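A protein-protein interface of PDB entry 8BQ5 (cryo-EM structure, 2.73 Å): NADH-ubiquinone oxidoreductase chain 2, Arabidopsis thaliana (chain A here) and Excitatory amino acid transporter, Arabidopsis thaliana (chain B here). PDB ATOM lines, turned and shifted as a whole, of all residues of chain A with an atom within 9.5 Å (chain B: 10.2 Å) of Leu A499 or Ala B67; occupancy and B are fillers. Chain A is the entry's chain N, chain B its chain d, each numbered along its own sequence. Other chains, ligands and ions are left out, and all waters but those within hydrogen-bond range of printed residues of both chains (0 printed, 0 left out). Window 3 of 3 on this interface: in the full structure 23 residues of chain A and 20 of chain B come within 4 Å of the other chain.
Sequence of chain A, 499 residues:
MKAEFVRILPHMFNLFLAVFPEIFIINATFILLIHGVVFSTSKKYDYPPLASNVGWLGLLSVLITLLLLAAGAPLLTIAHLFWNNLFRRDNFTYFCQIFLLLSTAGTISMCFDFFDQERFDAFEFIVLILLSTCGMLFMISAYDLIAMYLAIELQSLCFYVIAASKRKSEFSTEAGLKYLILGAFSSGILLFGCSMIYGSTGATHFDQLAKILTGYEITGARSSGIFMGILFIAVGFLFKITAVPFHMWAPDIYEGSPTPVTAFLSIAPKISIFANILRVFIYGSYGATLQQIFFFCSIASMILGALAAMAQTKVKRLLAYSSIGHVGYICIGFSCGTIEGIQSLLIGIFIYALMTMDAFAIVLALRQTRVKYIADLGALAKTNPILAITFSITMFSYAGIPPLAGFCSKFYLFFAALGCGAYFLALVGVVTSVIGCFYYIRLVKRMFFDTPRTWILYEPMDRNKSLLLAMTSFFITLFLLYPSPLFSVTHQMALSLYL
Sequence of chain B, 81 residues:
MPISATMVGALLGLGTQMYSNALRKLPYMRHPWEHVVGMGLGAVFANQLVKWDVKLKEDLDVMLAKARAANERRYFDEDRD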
ATOM      1  N   ASP A  90     -17.976 -17.911 -42.334  1.00  0.00           N
ATOM      2  CA  ASP A  90     -17.810 -18.834 -41.217  1.00  0.00           C
ATOM      3  C   ASP A  90     -19.110 -19.611 -41.034  1.00  0.00           C
ATOM      4  O   ASP A  90     -19.967 -19.636 -41.922  1.00  0.00           O
ATOM      5  CB  ASP A  90     -17.387 -18.081 -39.948  1.00  0.00           C
ATOM      6  CG  ASP A  90     -18.206 -16.829 -39.707  1.00  0.00           C
ATOM      7  OD1 ASP A  90     -19.412 -16.951 -39.411  1.00  0.00           O
ATOM      8  OD2 ASP A  90     -17.640 -15.721 -39.806  1.00  0.00           O
ATOM      9  N   ASN A  91     -19.252 -20.271 -39.878  1.00  0.00           N
ATOM     10  CA  ASN A  91     -20.462 -21.044 -39.604  1.00  0.00           C
ATOM     11  C   ASN A  91     -21.692 -20.146 -39.542  1.00  0.00           C
ATOM     12  O   ASN A  91     -22.752 -20.478 -40.097  1.00  0.00           O
ATOM     13  CB  ASN A  91     -20.312 -21.807 -38.287  1.00  0.00           C
ATOM     14  CG  ASN A  91     -19.468 -23.056 -38.422  1.00  0.00           C
ATOM     15  OD1 ASN A  91     -19.126 -23.477 -39.526  1.00  0.00           O
ATOM     16  ND2 ASN A  91     -19.134 -23.662 -37.291  1.00  0.00           N
ATOM     17  N   PHE A  92     -21.564 -19.006 -38.861  1.00  0.00           N
ATOM     18  CA  PHE A  92     -22.690 -18.099 -38.674  1.00  0.00           C
ATOM     19  C   PHE A  92     -23.217 -17.604 -40.013  1.00  0.00           C
ATOM     20  O   PHE A  92     -24.425 -17.661 -40.282  1.00  0.00           O
ATOM     21  CB  PHE A  92     -22.249 -16.936 -37.780  1.00  0.00           C
ATOM     22  CG  PHE A  92     -23.277 -15.860 -37.619  1.00  0.00           C
ATOM     23  CD1 PHE A  92     -24.356 -16.037 -36.772  1.00  0.00           C
ATOM     24  CD2 PHE A  92     -23.150 -14.658 -38.292  1.00  0.00           C
ATOM     25  CE1 PHE A  92     -25.300 -15.045 -36.618  1.00  0.00           C
ATOM     26  CE2 PHE A  92     -24.091 -13.661 -38.139  1.00  0.00           C
ATOM     27  CZ  PHE A  92     -25.166 -13.855 -37.301  1.00  0.00           C
ATOM     28  N   ILE A 282     -21.656  -6.974 -31.448  1.00  0.00           N
ATOM     29  CA  ILE A 282     -21.337  -8.092 -30.514  1.00  0.00           C
ATOM     30  C   ILE A 282     -19.863  -8.436 -30.726  1.00  0.00           C
ATOM     31  O   ILE A 282     -19.103  -8.382 -29.741  1.00  0.00           O
ATOM     32  CB  ILE A 282     -22.290  -9.283 -30.763  1.00  0.00           C
ATOM     33  CG1 ILE A 282     -23.601  -9.133 -29.986  1.00  0.00           C
ATOM     34  CG2 ILE A 282     -21.616 -10.616 -30.480  1.00  0.00           C
ATOM     35  CD1 ILE A 282     -23.424  -8.942 -28.497  1.00  0.00           C
ATOM     36  N   TYR A 283     -19.471  -8.684 -31.982  1.00  0.00           N
ATOM     37  CA  TYR A 283     -18.057  -8.965 -32.339  1.00  0.00           C
ATOM     38  C   TYR A 283     -17.184  -7.757 -31.998  1.00  0.00           C
ATOM     39  O   TYR A 283     -15.948  -7.912 -31.966  1.00  0.00           O
ATOM     40  CB  TYR A 283     -17.987  -9.164 -33.851  1.00  0.00           C
ATOM     41  CG  TYR A 283     -17.194 -10.333 -34.375  1.00  0.00           C
ATOM     42  CD1 TYR A 283     -15.924 -10.614 -33.906  1.00  0.00           C
ATOM     43  CD2 TYR A 283     -17.698 -11.125 -35.394  1.00  0.00           C
ATOM     44  CE1 TYR A 283     -15.191 -11.674 -34.409  1.00  0.00           C
ATOM     45  CE2 TYR A 283     -16.978 -12.189 -35.910  1.00  0.00           C
ATOM     46  CZ  TYR A 283     -15.716 -12.465 -35.415  1.00  0.00           C
ATOM     47  OH  TYR A 283     -14.996 -13.513 -35.911  1.00  0.00           O
ATOM     48  N   ILE A 339     -24.791 -15.223 -24.439  1.00  0.00           N
ATOM     49  CA  ILE A 339     -24.836 -16.236 -25.536  1.00  0.00           C
ATOM     50  C   ILE A 339     -26.292 -16.677 -25.726  1.00  0.00           C
ATOM     51  O   ILE A 339     -26.722 -16.764 -26.894  1.00  0.00           O
ATOM     52  CB  ILE A 339     -23.878 -17.410 -25.252  1.00  0.00           C
ATOM     53  CG1 ILE A 339     -22.449 -17.069 -25.676  1.00  0.00           C
ATOM     54  CG2 ILE A 339     -24.349 -18.704 -25.899  1.00  0.00           C
ATOM     55  CD1 ILE A 339     -22.227 -17.144 -27.164  1.00  0.00           C
ATOM     56  N   HIS A 491     -27.471 -22.343 -31.162  1.00  0.00           N
ATOM     57  CA  HIS A 491     -26.365 -22.286 -30.210  1.00  0.00           C
ATOM     58  C   HIS A 491     -25.024 -22.344 -30.930  1.00  0.00           C
ATOM     59  O   HIS A 491     -24.088 -21.607 -30.587  1.00  0.00           O
ATOM     60  CB  HIS A 491     -26.484 -23.430 -29.204  1.00  0.00           C
ATOM     61  CG  HIS A 491     -25.669 -23.232 -27.965  1.00  0.00           C
ATOM     62  ND1 HIS A 491     -25.541 -24.202 -26.995  1.00  0.00           N
ATOM     63  CD2 HIS A 491     -24.951 -22.170 -27.533  1.00  0.00           C
ATOM     64  CE1 HIS A 491     -24.774 -23.748 -26.020  1.00  0.00           C
ATOM     65  NE2 HIS A 491     -24.402 -22.517 -26.323  1.00  0.00           N
ATOM     66  N   GLN A 492     -24.921 -23.217 -31.933  1.00  0.00           N
ATOM     67  CA  GLN A 492     -23.725 -23.293 -32.763  1.00  0.00           C
ATOM     68  C   GLN A 492     -23.394 -21.941 -33.382  1.00  0.00           C
ATOM     69  O   GLN A 492     -22.243 -21.494 -33.345  1.00  0.00           O
ATOM     70  CB  GLN A 492     -23.934 -24.344 -33.849  1.00  0.00           C
ATOM     71  CG  GLN A 492     -22.698 -24.710 -34.626  1.00  0.00           C
ATOM     72  CD  GLN A 492     -22.877 -25.998 -35.398  1.00  0.00           C
ATOM     73  OE1 GLN A 492     -23.417 -26.976 -34.880  1.00  0.00           O
ATOM     74  NE2 GLN A 492     -22.435 -26.003 -36.650  1.00  0.00           N
ATOM     75  N   MET A 493     -24.395 -21.276 -33.962  1.00  0.00           N
ATOM     76  CA  MET A 493     -24.153 -19.982 -34.596  1.00  0.00           C
ATOM     77  C   MET A 493     -23.713 -18.936 -33.579  1.00  0.00           C
ATOM     78  O   MET A 493     -22.731 -18.207 -33.800  1.00  0.00           O
ATOM     79  CB  MET A 493     -25.417 -19.513 -35.306  1.00  0.00           C
ATOM     80  CG  MET A 493     -25.558 -20.002 -36.720  1.00  0.00           C
ATOM     81  SD  MET A 493     -27.292 -20.322 -37.058  1.00  0.00           S
ATOM     82  CE  MET A 493     -27.794 -18.686 -37.570  1.00  0.00           C
ATOM     83  N   ALA A 494     -24.407 -18.859 -32.447  1.00  0.00           N
ATOM     84  CA  ALA A 494     -24.076 -17.857 -31.403  1.00  0.00           C
ATOM     85  C   ALA A 494     -22.590 -17.929 -31.030  1.00  0.00           C
ATOM     86  O   ALA A 494     -21.994 -16.858 -30.854  1.00  0.00           O
ATOM     87  CB  ALA A 494     -24.959 -18.064 -30.202  1.00  0.00           C
ATOM     88  N   LEU A 495     -22.015 -19.132 -30.937  1.00  0.00           N
ATOM     89  CA  LEU A 495     -20.597 -19.298 -30.513  1.00  0.00           C
ATOM     90  C   LEU A 495     -19.641 -19.015 -31.673  1.00  0.00           C
ATOM     91  O   LEU A 495     -18.557 -18.486 -31.405  1.00  0.00           O
ATOM     92  CB  LEU A 495     -20.404 -20.722 -29.983  1.00  0.00           C
ATOM     93  CG  LEU A 495     -21.018 -21.025 -28.617  1.00  0.00           C
ATOM     94  CD1 LEU A 495     -21.210 -22.523 -28.441  1.00  0.00           C
ATOM     95  CD2 LEU A 495     -20.148 -20.477 -27.499  1.00  0.00           C
ATOM     96  N   SER A 496     -20.029 -19.344 -32.908  1.00  0.00           N
ATOM     97  CA  SER A 496     -19.183 -19.064 -34.096  1.00  0.00           C
ATOM     98  C   SER A 496     -18.871 -17.565 -34.190  1.00  0.00           C
ATOM     99  O   SER A 496     -17.785 -17.240 -34.703  1.00  0.00           O
ATOM    100  CB  SER A 496     -19.826 -19.590 -35.350  1.00  0.00           C
ATOM    101  OG  SER A 496     -20.126 -20.968 -35.201  1.00  0.00           O
ATOM    102  N   LEU A 497     -19.755 -16.708 -33.672  1.00  0.00           N
ATOM    103  CA  LEU A 497     -19.512 -15.240 -33.669  1.00  0.00           C
ATOM    104  C   LEU A 497     -18.246 -14.908 -32.875  1.00  0.00           C
ATOM    105  O   LEU A 497     -17.453 -14.098 -33.369  1.00  0.00           O
ATOM    106  CB  LEU A 497     -20.720 -14.533 -33.052  1.00  0.00           C
ATOM    107  CG  LEU A 497     -21.916 -14.316 -33.976  1.00  0.00           C
ATOM    108  CD1 LEU A 497     -23.087 -13.734 -33.200  1.00  0.00           C
ATOM    109  CD2 LEU A 497     -21.543 -13.403 -35.133  1.00  0.00           C
ATOM    110  N   TYR A 498     -18.070 -15.493 -31.688  1.00  0.00           N
ATOM    111  CA  TYR A 498     -16.920 -15.132 -30.816  1.00  0.00           C
ATOM    112  C   TYR A 498     -15.733 -16.046 -31.113  1.00  0.00           C
ATOM    113  O   TYR A 498     -14.684 -15.542 -31.512  1.00  0.00           O
ATOM    114  CB  TYR A 498     -17.306 -15.247 -29.342  1.00  0.00           C
ATOM    115  CG  TYR A 498     -18.436 -14.363 -28.881  1.00  0.00           C
ATOM    116  CD1 TYR A 498     -19.721 -14.861 -28.745  1.00  0.00           C
ATOM    117  CD2 TYR A 498     -18.216 -13.037 -28.550  1.00  0.00           C
ATOM    118  CE1 TYR A 498     -20.762 -14.059 -28.308  1.00  0.00           C
ATOM    119  CE2 TYR A 498     -19.245 -12.222 -28.109  1.00  0.00           C
ATOM    120  CZ  TYR A 498     -20.523 -12.737 -27.983  1.00  0.00           C
ATOM    121  OH  TYR A 498     -21.542 -11.940 -27.552  1.00  0.00           O
ATOM    122  N   LEU A 499     -15.917 -17.351 -30.948  1.00  0.00           N
ATOM    123  CA  LEU A 499     -14.816 -18.325 -31.164  1.00  0.00           C
ATOM    124  C   LEU A 499     -15.027 -19.056 -32.494  1.00  0.00           C
ATOM    125  O   LEU A 499     -15.834 -20.004 -32.509  1.00  0.00           O
ATOM    126  CB  LEU A 499     -14.764 -19.313 -29.993  1.00  0.00           C
ATOM    127  CG  LEU A 499     -16.004 -20.185 -29.785  1.00  0.00           C
ATOM    128  CD1 LEU A 499     -16.002 -21.357 -30.752  1.00  0.00           C
ATOM    129  CD2 LEU A 499     -16.092 -20.672 -28.348  1.00  0.00           C
ATOM    130  N   ASP B  59     -21.150 -31.487 -33.302  1.00  0.00           N
ATOM    131  CA  ASP B  59     -20.352 -30.291 -33.565  1.00  0.00           C
ATOM    132  C   ASP B  59     -20.427 -29.298 -32.406  1.00  0.00           C
ATOM    133  O   ASP B  59     -19.414 -28.688 -32.023  1.00  0.00           O
ATOM    134  CB  ASP B  59     -20.814 -29.645 -34.869  1.00  0.00           C
ATOM    135  CG  ASP B  59     -20.600 -30.549 -36.067  1.00  0.00           C
ATOM    136  OD1 ASP B  59     -19.634 -31.340 -36.044  1.00  0.00           O
ATOM    137  OD2 ASP B  59     -21.397 -30.476 -37.025  1.00  0.00           O
ATOM    138  N   LEU B  60     -21.625 -29.121 -31.841  1.00  0.00           N
ATOM    139  CA  LEU B  60     -21.791 -28.221 -30.709  1.00  0.00           C
ATOM    140  C   LEU B  60     -20.956 -28.660 -29.517  1.00  0.00           C
ATOM    141  O   LEU B  60     -20.459 -27.812 -28.768  1.00  0.00           O
ATOM    142  CB  LEU B  60     -23.266 -28.131 -30.319  1.00  0.00           C
ATOM    143  CG  LEU B  60     -23.596 -27.127 -29.213  1.00  0.00           C
ATOM    144  CD1 LEU B  60     -23.216 -25.712 -29.619  1.00  0.00           C
ATOM    145  CD2 LEU B  60     -25.063 -27.203 -28.820  1.00  0.00           C
ATOM    146  N   ASP B  61     -20.795 -29.968 -29.317  1.00  0.00           N
ATOM    147  CA  ASP B  61     -19.983 -30.434 -28.196  1.00  0.00           C
ATOM    148  C   ASP B  61     -18.535 -29.968 -28.331  1.00  0.00           C
ATOM    149  O   ASP B  61     -17.939 -29.465 -27.371  1.00  0.00           O
ATOM    150  CB  ASP B  61     -20.061 -31.956 -28.089  1.00  0.00           C
ATOM    151  CG  ASP B  61     -21.410 -32.432 -27.590  1.00  0.00           C
ATOM    152  OD1 ASP B  61     -22.213 -31.583 -27.150  1.00  0.00           O
ATOM    153  OD2 ASP B  61     -21.670 -33.651 -27.642  1.00  0.00           O
ATOM    154  N   VAL B  62     -17.963 -30.099 -29.531  1.00  0.00           N
ATOM    155  CA  VAL B  62     -16.587 -29.662 -29.756  1.00  0.00           C
ATOM    156  C   VAL B  62     -16.464 -28.154 -29.574  1.00  0.00           C
ATOM    157  O   VAL B  62     -15.494 -27.654 -28.980  1.00  0.00           O
ATOM    158  CB  VAL B  62     -16.111 -30.094 -31.153  1.00  0.00           C
ATOM    159  CG1 VAL B  62     -14.621 -29.845 -31.301  1.00  0.00           C
ATOM    160  CG2 VAL B  62     -16.444 -31.554 -31.398  1.00  0.00           C
ATOM    161  N   MET B  63     -17.432 -27.400 -30.099  1.00  0.00           N
ATOM    162  CA  MET B  63     -17.321 -25.950 -29.988  1.00  0.00           C
ATOM    163  C   MET B  63     -17.472 -25.484 -28.541  1.00  0.00           C
ATOM    164  O   MET B  63     -16.792 -24.542 -28.114  1.00  0.00           O
ATOM    165  CB  MET B  63     -18.333 -25.275 -30.907  1.00  0.00           C
ATOM    166  CG  MET B  63     -17.895 -25.324 -32.365  1.00  0.00           C
ATOM    167  SD  MET B  63     -18.928 -24.349 -33.470  1.00  0.00           S
ATOM    168  CE  MET B  63     -19.681 -23.222 -32.306  1.00  0.00           C
ATOM    169  N   LEU B  64     -18.336 -26.141 -27.762  1.00  0.00           N
ATOM    170  CA  LEU B  64     -18.424 -25.809 -26.345  1.00  0.00           C
ATOM    171  C   LEU B  64     -17.153 -26.204 -25.607  1.00  0.00           C
ATOM    172  O   LEU B  64     -16.761 -25.543 -24.640  1.00  0.00           O
ATOM    173  CB  LEU B  64     -19.633 -26.481 -25.702  1.00  0.00           C
ATOM    174  CG  LEU B  64     -20.959 -25.788 -25.978  1.00  0.00           C
ATOM    175  CD1 LEU B  64     -22.084 -26.800 -26.019  1.00  0.00           C
ATOM    176  CD2 LEU B  64     -21.198 -24.708 -24.961  1.00  0.00           C
ATOM    177  N   ALA B  65     -16.502 -27.286 -26.039  1.00  0.00           N
ATOM    178  CA  ALA B  65     -15.208 -27.636 -25.464  1.00  0.00           C
ATOM    179  C   ALA B  65     -14.205 -26.508 -25.670  1.00  0.00           C
ATOM    180  O   ALA B  65     -13.489 -26.116 -24.738  1.00  0.00           O
ATOM    181  CB  ALA B  65     -14.695 -28.937 -26.082  1.00  0.00           C
ATOM    182  N   LYS B  66     -14.156 -25.963 -26.889  1.00  0.00           N
ATOM    183  CA  LYS B  66     -13.254 -24.844 -27.158  1.00  0.00           C
ATOM    184  C   LYS B  66     -13.617 -23.614 -26.329  1.00  0.00           C
ATOM    185  O   LYS B  66     -12.733 -22.937 -25.787  1.00  0.00           O
ATOM    186  CB  LYS B  66     -13.264 -24.499 -28.646  1.00  0.00           C
ATOM    187  CG  LYS B  66     -12.852 -25.637 -29.556  1.00  0.00           C
ATOM    188  CD  LYS B  66     -12.801 -25.174 -31.001  1.00  0.00           C
ATOM    189  CE  LYS B  66     -12.178 -26.225 -31.902  1.00  0.00           C
ATOM    190  NZ  LYS B  66     -11.709 -25.631 -33.187  1.00  0.00           N
ATOM    191  N   ALA B  67     -14.913 -23.304 -26.232  1.00  0.00           N
ATOM    192  CA  ALA B  67     -15.341 -22.150 -25.447  1.00  0.00           C
ATOM    193  C   ALA B  67     -14.942 -22.298 -23.986  1.00  0.00           C
ATOM    194  O   ALA B  67     -14.435 -21.351 -23.371  1.00  0.00           O
ATOM    195  CB  ALA B  67     -16.852 -21.960 -25.568  1.00  0.00           C
ATOM    196  N   ARG B  68     -15.160 -23.484 -23.414  1.00  0.00           N
ATOM    197  CA  ARG B  68     -14.811 -23.706 -22.017  1.00  0.00           C
ATOM    198  C   ARG B  68     -13.304 -23.653 -21.806  1.00  0.00           C
ATOM    199  O   ARG B  68     -12.838 -23.149 -20.781  1.00  0.00           O
ATOM    200  CB  ARG B  68     -15.378 -25.039 -21.531  1.00  0.00           C
ATOM    201  CG  ARG B  68     -16.674 -24.895 -20.749  1.00  0.00           C
ATOM    202  CD  ARG B  68     -17.373 -26.226 -20.570  1.00  0.00           C
ATOM    203  NE  ARG B  68     -17.834 -26.776 -21.837  1.00  0.00           N
ATOM    204  CZ  ARG B  68     -17.871 -28.070 -22.120  1.00  0.00           C
ATOM    205  NH1 ARG B  68     -17.497 -28.981 -21.238  1.00  0.00           N
ATOM    206  NH2 ARG B  68     -18.294 -28.460 -23.319  1.00  0.00           N
ATOM    207  N   ALA B  69     -12.521 -24.169 -22.760  1.00  0.00           N
ATOM    208  CA  ALA B  69     -11.070 -24.055 -22.641  1.00  0.00           C
ATOM    209  C   ALA B  69     -10.634 -22.593 -22.623  1.00  0.00           C
ATOM    210  O   ALA B  69      -9.819 -22.183 -21.781  1.00  0.00           O
ATOM    211  CB  ALA B  69     -10.385 -24.806 -23.782  1.00  0.00           C
ATOM    212  N   ALA B  70     -11.188 -21.785 -23.531  1.00  0.00           N
ATOM    213  CA  ALA B  70     -10.846 -20.367 -23.554  1.00  0.00           C
ATOM    214  C   ALA B  70     -11.236 -19.686 -22.247  1.00  0.00           C
ATOM    215  O   ALA B  70     -10.474 -18.875 -21.709  1.00  0.00           O
ATOM    216  CB  ALA B  70     -11.518 -19.680 -24.742  1.00  0.00           C
ATOM    217  N   ASN B  71     -12.418 -20.009 -21.716  1.00  0.00           N
ATOM    218  CA  ASN B  71     -12.870 -19.378 -20.479  1.00  0.00           C
ATOM    219  C   ASN B  71     -12.039 -19.829 -19.280  1.00  0.00           C
ATOM    220  O   ASN B  71     -11.833 -19.056 -18.337  1.00  0.00           O
ATOM    221  CB  ASN B  71     -14.353 -19.675 -20.257  1.00  0.00           C
ATOM    222  CG  ASN B  71     -14.927 -18.928 -19.071  1.00  0.00           C
ATOM    223  OD1 ASN B  71     -14.720 -17.724 -18.920  1.00  0.00           O
ATOM    224  ND2 ASN B  71     -15.659 -19.639 -18.223  1.00  0.00           N
ATOM    225  N   GLU B  72     -11.563 -21.078 -19.291  1.00  0.00           N
ATOM    226  CA  GLU B  72     -10.710 -21.569 -18.215  1.00  0.00           C
ATOM    227  C   GLU B  72      -9.294 -21.028 -18.317  1.00  0.00           C
ATOM    228  O   GLU B  72      -8.538 -21.110 -17.342  1.00  0.00           O
ATOM    229  CB  GLU B  72     -10.670 -23.098 -18.221  1.00  0.00           C
ATOM    230  CG  GLU B  72     -11.986 -23.769 -17.878  1.00  0.00           C
ATOM    231  CD  GLU B  72     -11.914 -25.278 -18.011  1.00  0.00           C
ATOM    232  OE1 GLU B  72     -10.877 -25.782 -18.489  1.00  0.00           O
ATOM    233  OE2 GLU B  72     -12.900 -25.958 -17.657  1.00  0.00           O
ATOM    234  N   ARG B  73      -8.910 -20.503 -19.483  1.00  0.00           N
ATOM    235  CA  ARG B  73      -7.610 -19.851 -19.606  1.00  0.00           C
ATOM    236  C   ARG B  73      -7.475 -18.623 -18.709  1.00  0.00           C
ATOM    237  O   ARG B  73      -6.347 -18.220 -18.400  1.00  0.00           O
ATOM    238  CB  ARG B  73      -7.363 -19.448 -21.059  1.00  0.00           C
ATOM    239  CG  ARG B  73      -6.990 -20.598 -21.976  1.00  0.00           C
ATOM    240  CD  ARG B  73      -5.742 -21.308 -21.491  1.00  0.00           C
ATOM    241  NE  ARG B  73      -4.547 -20.498 -21.687  1.00  0.00           N
ATOM    242  CZ  ARG B  73      -3.851 -20.443 -22.814  1.00  0.00           C
ATOM    243  NH1 ARG B  73      -4.210 -21.135 -23.883  1.00  0.00           N
ATOM    244  NH2 ARG B  73      -2.768 -19.674 -22.871  1.00  0.00           N
ATOM    245  N   ARG B  74      -8.590 -18.018 -18.286  1.00  0.00           N
ATOM    246  CA  ARG B  74      -8.516 -16.773 -17.522  1.00  0.00           C
ATOM    247  C   ARG B  74      -7.910 -16.987 -16.140  1.00  0.00           C
ATOM    248  O   ARG B  74      -7.305 -16.070 -15.572  1.00  0.00           O
ATOM    249  CB  ARG B  74      -9.902 -16.140 -17.395  1.00  0.00           C
ATOM    250  CG  ARG B  74      -9.865 -14.625 -17.256  1.00  0.00           C
ATOM    251  CD  ARG B  74     -11.221 -14.041 -16.898  1.00  0.00           C
ATOM    252  NE  ARG B  74     -12.202 -14.244 -17.956  1.00  0.00           N
ATOM    253  CZ  ARG B  74     -13.277 -15.011 -17.840  1.00  0.00           C
ATOM    254  NH1 ARG B  74     -13.555 -15.643 -16.712  1.00  0.00           N
ATOM    255  NH2 ARG B  74     -14.096 -15.142 -18.880  1.00  0.00           N
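The backbone carbonyl oxygen (O) of Gln A492 is in hydrogen-bond range of the side-chain hydroxyl (OG) of Ser A496, 2.9 Å away. The backbone carbonyl oxygen of Leu B64 is in hydrogen-bond range of the guanidinium group of Arg B68 (3.2 Å).
Asn A91 touches Met B63 (ND2 to SD, 3.9 Å). ND1 of His A491 touches CD2 of Leu B60 (3.5 Å). His A491 touches Leu B64 (CE1 to CD2, 3.9 Å). Asp B59 touches Gln A492 (CB to OE1, 3.7 Å). N of Gln A492 touches CD1 of Leu B60 (3.8 Å). O of Gln A492 touches CE of Met B63, 3.3 Å away. Leu A495 touches Leu B60. CB of Leu A495 touches CE of Met B63, 3.5 Å away. OG of Ser A496 touches CE of Met B63, at 3.7 Å. CB of Ala B67 touches CD2 of Leu A499, 3.2 Å away.
Of the printed residues of chain B, His A491 touches Leu B60 and Leu B64. Printed residues of chain B within 4 Å of Gln A492: Asp B59 (3.7 Å), Leu B60 (3.8 Å) and Met B63 (3.3 Å). Of the printed residues of chain B, Ser A496 touches Met B63. Of chain B, only Met B63 (3.9 Å) and Ala B67 (3.2 Å) come within 4 Å of Leu A499. Printed residues of chain A within 4 Å of Asp B59: Gln A492 (3.7 Å). Of the printed residues of chain A, Leu B60 touches His A491, Gln A492 and Leu A495. Val B62 touches none of the printed residues of chain A. Printed residues of chain A within 4 Å of Leu B64: His A491. Of chain A, only Leu A499 comes within 4 Å of Ala B67. No residue of chain A comes within 4 Å of Ala B69. No residue of chain A comes within 4 Å of Ala B70. The nearest residue of chain A that does not touch Ala B67 is Leu A495 (4.1 Å). The nearest printed residue of chain B that does not touch Leu A495 is Leu B64 (4.1 Å).
Of the 16 printed residues of chain B, 5 touch a printed residue of chain A. Hydrophobic or aromatic side chains of chain B that line the printed part of chain A: Leu B60, Met B63, Leu B64 and Ala B67. Of the 15 printed residues of chain A, 6 touch a printed residue of chain B. Printed residues of chain A that touch a printed residue of chain B: Asn A91, His A491, Gln A492, Leu A495, Ser A496 and Leu A499. Among the printed residues, 11 pairs touch across the chains. Among the printed residues, no Asp or Glu carboxylate lies within 4 Å of a Lys or Arg side-chain nitrogen of the other chain.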
